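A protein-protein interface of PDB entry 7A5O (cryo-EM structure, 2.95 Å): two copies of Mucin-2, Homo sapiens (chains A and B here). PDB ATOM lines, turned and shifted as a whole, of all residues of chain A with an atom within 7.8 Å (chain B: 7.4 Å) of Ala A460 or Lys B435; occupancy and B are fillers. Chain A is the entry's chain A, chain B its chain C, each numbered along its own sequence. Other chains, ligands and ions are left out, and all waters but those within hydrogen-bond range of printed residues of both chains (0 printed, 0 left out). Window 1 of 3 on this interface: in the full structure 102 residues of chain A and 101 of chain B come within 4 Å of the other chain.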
ATOM      1  N   HIS A 457      -9.289   9.310  10.973  1.00  0.00           N
ATOM      2  CA  HIS A 457      -8.450   9.170  12.163  1.00  0.00           C
ATOM      3  C   HIS A 457      -7.218   8.375  11.746  1.00  0.00           C
ATOM      4  O   HIS A 457      -7.247   7.142  11.734  1.00  0.00           O
ATOM      5  CB  HIS A 457      -9.203   8.477  13.289  1.00  0.00           C
ATOM      6  CG  HIS A 457      -8.408   8.318  14.546  1.00  0.00           C
ATOM      7  ND1 HIS A 457      -8.165   9.360  15.414  1.00  0.00           N
ATOM      8  CD2 HIS A 457      -7.792   7.235  15.079  1.00  0.00           C
ATOM      9  CE1 HIS A 457      -7.440   8.925  16.429  1.00  0.00           C
ATOM     10  NE2 HIS A 457      -7.200   7.640  16.250  1.00  0.00           N
ATOM     11  N   VAL A 458      -6.143   9.079  11.407  1.00  0.00           N
ATOM     12  CA  VAL A 458      -4.919   8.470  10.899  1.00  0.00           C
ATOM     13  C   VAL A 458      -3.877   8.485  12.007  1.00  0.00           C
ATOM     14  O   VAL A 458      -3.590   9.541  12.580  1.00  0.00           O
ATOM     15  CB  VAL A 458      -4.408   9.204   9.647  1.00  0.00           C
ATOM     16  CG1 VAL A 458      -3.080   8.632   9.192  1.00  0.00           C
ATOM     17  CG2 VAL A 458      -5.431   9.118   8.532  1.00  0.00           C
ATOM     18  N   THR A 459      -3.319   7.319  12.311  1.00  0.00           N
ATOM     19  CA  THR A 459      -2.302   7.167  13.342  1.00  0.00           C
ATOM     20  C   THR A 459      -1.052   6.533  12.737  1.00  0.00           C
ATOM     21  O   THR A 459      -0.905   6.434  11.516  1.00  0.00           O
ATOM     22  CB  THR A 459      -2.817   6.331  14.516  1.00  0.00           C
ATOM     23  OG1 THR A 459      -3.171   5.022  14.054  1.00  0.00           O
ATOM     24  CG2 THR A 459      -4.021   6.988  15.174  1.00  0.00           C
ATOM     25  N   ALA A 460      -0.141   6.109  13.612  1.00  0.00           N
ATOM     26  CA  ALA A 460       1.122   5.538  13.159  1.00  0.00           C
ATOM     27  C   ALA A 460       0.978   4.076  12.756  1.00  0.00           C
ATOM     28  O   ALA A 460       1.636   3.626  11.812  1.00  0.00           O
ATOM     29  CB  ALA A 460       2.183   5.681  14.249  1.00  0.00           C
ATOM     30  N   SER A 461       0.129   3.318  13.453  1.00  0.00           N
ATOM     31  CA  SER A 461      -0.004   1.892  13.195  1.00  0.00           C
ATOM     32  C   SER A 461      -1.263   1.513  12.432  1.00  0.00           C
ATOM     33  O   SER A 461      -1.279   0.450  11.804  1.00  0.00           O
ATOM     34  CB  SER A 461       0.035   1.104  14.511  1.00  0.00           C
ATOM     35  OG  SER A 461      -1.091   1.396  15.315  1.00  0.00           O
ATOM     36  N   PHE A 462      -2.308   2.336  12.465  1.00  0.00           N
ATOM     37  CA  PHE A 462      -3.499   2.067  11.673  1.00  0.00           C
ATOM     38  C   PHE A 462      -4.168   3.386  11.317  1.00  0.00           C
ATOM     39  O   PHE A 462      -3.758   4.457  11.768  1.00  0.00           O
ATOM     40  CB  PHE A 462      -4.474   1.126  12.404  1.00  0.00           C
ATOM     41  CG  PHE A 462      -5.087   1.708  13.649  1.00  0.00           C
ATOM     42  CD1 PHE A 462      -4.435   1.609  14.864  1.00  0.00           C
ATOM     43  CD2 PHE A 462      -6.346   2.287  13.616  1.00  0.00           C
ATOM     44  CE1 PHE A 462      -4.998   2.129  16.011  1.00  0.00           C
ATOM     45  CE2 PHE A 462      -6.914   2.808  14.755  1.00  0.00           C
ATOM     46  CZ  PHE A 462      -6.240   2.726  15.955  1.00  0.00           C
ATOM     47  N   SER A 463      -5.217   3.291  10.502  1.00  0.00           N
ATOM     48  CA  SER A 463      -5.993   4.454  10.100  1.00  0.00           C
ATOM     49  C   SER A 463      -7.382   3.997   9.685  1.00  0.00           C
ATOM     50  O   SER A 463      -7.531   2.947   9.061  1.00  0.00           O
ATOM     51  CB  SER A 463      -5.316   5.207   8.952  1.00  0.00           C
ATOM     52  OG  SER A 463      -5.295   4.423   7.775  1.00  0.00           O
ATOM     53  N   SER A 475      -7.218   0.359   7.539  1.00  0.00           N
ATOM     54  CA  SER A 475      -5.960  -0.210   7.087  1.00  0.00           C
ATOM     55  C   SER A 475      -4.987  -0.284   8.254  1.00  0.00           C
ATOM     56  O   SER A 475      -4.919   0.633   9.074  1.00  0.00           O
ATOM     57  CB  SER A 475      -5.362   0.619   5.952  1.00  0.00           C
ATOM     58  OG  SER A 475      -4.122   0.082   5.536  1.00  0.00           O
ATOM     59  N   MET A 476      -4.243  -1.381   8.330  1.00  0.00           N
ATOM     60  CA  MET A 476      -3.256  -1.583   9.377  1.00  0.00           C
ATOM     61  C   MET A 476      -1.879  -1.801   8.768  1.00  0.00           C
ATOM     62  O   MET A 476      -1.749  -2.310   7.653  1.00  0.00           O
ATOM     63  CB  MET A 476      -3.602  -2.775  10.257  1.00  0.00           C
ATOM     64  CG  MET A 476      -4.833  -2.598  11.105  1.00  0.00           C
ATOM     65  SD  MET A 476      -5.171  -4.110  12.006  1.00  0.00           S
ATOM     66  CE  MET A 476      -3.797  -4.101  13.143  1.00  0.00           C
ATOM     67  N   ALA A 477      -0.851  -1.422   9.525  1.00  0.00           N
ATOM     68  CA  ALA A 477       0.527  -1.583   9.087  1.00  0.00           C
ATOM     69  C   ALA A 477       1.009  -3.021   9.176  1.00  0.00           C
ATOM     70  O   ALA A 477       2.048  -3.344   8.593  1.00  0.00           O
ATOM     71  CB  ALA A 477       1.446  -0.686   9.910  1.00  0.00           C
ATOM     72  N   LEU B 430       6.024  15.503  20.017  1.00  0.00           N
ATOM     73  CA  LEU B 430       6.425  14.443  19.097  1.00  0.00           C
ATOM     74  C   LEU B 430       6.729  13.206  19.933  1.00  0.00           C
ATOM     75  O   LEU B 430       7.839  13.040  20.435  1.00  0.00           O
ATOM     76  CB  LEU B 430       7.630  14.867  18.281  1.00  0.00           C
ATOM     77  CG  LEU B 430       7.430  16.016  17.300  1.00  0.00           C
ATOM     78  CD1 LEU B 430       8.756  16.445  16.758  1.00  0.00           C
ATOM     79  CD2 LEU B 430       6.557  15.572  16.166  1.00  0.00           C
ATOM     80  N   ALA B 431       5.738  12.332  20.072  1.00  0.00           N
ATOM     81  CA  ALA B 431       5.820  11.194  20.973  1.00  0.00           C
ATOM     82  C   ALA B 431       5.645   9.890  20.207  1.00  0.00           C
ATOM     83  O   ALA B 431       5.360   9.885  19.007  1.00  0.00           O
ATOM     84  CB  ALA B 431       4.767  11.301  22.079  1.00  0.00           C
ATOM     85  N   ASP B 432       5.820   8.784  20.943  1.00  0.00           N
ATOM     86  CA  ASP B 432       5.674   7.402  20.469  1.00  0.00           C
ATOM     87  C   ASP B 432       6.617   7.116  19.295  1.00  0.00           C
ATOM     88  O   ASP B 432       6.196   6.876  18.160  1.00  0.00           O
ATOM     89  CB  ASP B 432       4.219   7.085  20.105  1.00  0.00           C
ATOM     90  N   LYS B 433       7.915   7.169  19.624  1.00  0.00           N
ATOM     91  CA  LYS B 433       9.034   7.022  18.683  1.00  0.00           C
ATOM     92  C   LYS B 433       8.968   8.046  17.553  1.00  0.00           C
ATOM     93  O   LYS B 433       9.335   7.748  16.413  1.00  0.00           O
ATOM     94  CB  LYS B 433       9.128   5.598  18.121  1.00  0.00           C
ATOM     95  N   LYS B 434       8.469   9.243  17.887  1.00  0.00           N
ATOM     96  CA  LYS B 434       8.432  10.425  17.021  1.00  0.00           C
ATOM     97  C   LYS B 434       7.618  10.204  15.748  1.00  0.00           C
ATOM     98  O   LYS B 434       7.862  10.848  14.727  1.00  0.00           O
ATOM     99  CB  LYS B 434       9.842  10.910  16.680  1.00  0.00           C
ATOM    100  CG  LYS B 434      10.594  11.418  17.890  1.00  0.00           C
ATOM    101  CD  LYS B 434      11.988  11.870  17.528  1.00  0.00           C
ATOM    102  CE  LYS B 434      11.915  13.145  16.732  1.00  0.00           C
ATOM    103  NZ  LYS B 434      11.367  14.214  17.593  1.00  0.00           N
ATOM    104  N   LYS B 435       6.636   9.306  15.799  1.00  0.00           N
ATOM    105  CA  LYS B 435       5.740   9.078  14.676  1.00  0.00           C
ATOM    106  C   LYS B 435       4.368   9.708  14.873  1.00  0.00           C
ATOM    107  O   LYS B 435       3.599   9.789  13.910  1.00  0.00           O
ATOM    108  CB  LYS B 435       5.579   7.574  14.425  1.00  0.00           C
ATOM    109  N   ASN B 436       4.048  10.149  16.087  1.00  0.00           N
ATOM    110  CA  ASN B 436       2.785  10.807  16.394  1.00  0.00           C
ATOM    111  C   ASN B 436       3.068  12.250  16.783  1.00  0.00           C
ATOM    112  O   ASN B 436       3.802  12.500  17.744  1.00  0.00           O
ATOM    113  CB  ASN B 436       2.051  10.086  17.523  1.00  0.00           C
ATOM    114  CG  ASN B 436       1.493   8.745  17.096  1.00  0.00           C
ATOM    115  OD1 ASN B 436       0.935   8.610  16.011  1.00  0.00           O
ATOM    116  ND2 ASN B 436       1.636   7.746  17.953  1.00  0.00           N
ATOM    117  N   ALA B 437       2.485  13.191  16.048  1.00  0.00           N
ATOM    118  CA  ALA B 437       2.632  14.613  16.324  1.00  0.00           C
ATOM    119  C   ALA B 437       1.319  15.144  16.873  1.00  0.00           C
ATOM    120  O   ALA B 437       0.273  14.994  16.234  1.00  0.00           O
ATOM    121  CB  ALA B 437       3.026  15.379  15.062  1.00  0.00           C
ATOM    122  N   LEU B 448      -4.314  15.781  16.116  1.00  0.00           N
ATOM    123  CA  LEU B 448      -3.345  14.705  15.967  1.00  0.00           C
ATOM    124  C   LEU B 448      -3.145  14.401  14.491  1.00  0.00           C
ATOM    125  O   LEU B 448      -4.095  13.996  13.812  1.00  0.00           O
ATOM    126  CB  LEU B 448      -3.826  13.454  16.698  1.00  0.00           C
ATOM    127  CG  LEU B 448      -2.992  12.177  16.602  1.00  0.00           C
ATOM    128  CD1 LEU B 448      -1.622  12.354  17.195  1.00  0.00           C
ATOM    129  CD2 LEU B 448      -3.715  11.029  17.278  1.00  0.00           C
ATOM    130  N   ASN B 449      -1.907  14.589  14.014  1.00  0.00           N
ATOM    131  CA  ASN B 449      -1.489  14.321  12.632  1.00  0.00           C
ATOM    132  C   ASN B 449      -2.343  15.095  11.630  1.00  0.00           C
ATOM    133  O   ASN B 449      -2.906  14.528  10.692  1.00  0.00           O
ATOM    134  CB  ASN B 449      -1.489  12.821  12.336  1.00  0.00           C
ATOM    135  CG  ASN B 449      -0.377  12.087  13.066  1.00  0.00           C
ATOM    136  OD1 ASN B 449       0.757  12.557  13.121  1.00  0.00           O
ATOM    137  ND2 ASN B 449      -0.703  10.942  13.650  1.00  0.00           N
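ND2 of Asn B449 sits at hydrogen-bond distance from O of Val A458, at 3.4 Å.
O of Asn B436 lies within hydrogen-bond range of N of Ala B431 (3.0 Å).
The backbone NH of Asn B449 lies within hydrogen-bond range of the backbone carbonyl oxygen of Ala B437, 3.1 Å away.
Ala A460 touches Lys B435 (CB to CB, 3.9 Å).
Ala A460 touches Asn B436.
Ala A460 touches just these residues of chain B: Lys B435 and Asn B436.
Printed residues of chain A within 4 Å of Lys B435: Ala A460 (3.9 Å).
Of the printed residues of chain A, Asn B436 touches Ala A460.
Printed residues of chain A within 4 Å of Asn B449: Val A458 (3.4 Å).
The nearest residue of chain B that does not touch Ala A460 is Asn B449 (4.9 Å).
The nearest printed residue of chain B that does not touch Val A458 is Leu B448 (4.6 Å).
Of the 10 printed residues of chain A, 2 touch a printed residue of chain B.
Printed residues of chain A that touch a printed residue of chain B: Val A458 and Ala A460.
Hydrophobic or aromatic side chains of chain A that line the printed part of chain B: Ala A460.
Of the 10 printed residues of chain B, 3 touch a printed residue of chain A.
Printed residues of chain B that touch a printed residue of chain A: Lys B435, Asn B436 and Asn B449.
Among the printed residues, 3 pairs touch across the chains.
Among the printed residues, no Asp or Glu carboxylate lies within 4 Å of a Lys or Arg side-chain nitrogen of the other chain.
No position is printed for both chains.
Of the 3 pairs that touch across the chains among the printed residues, none has its exchanged pair printed and touching as well.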
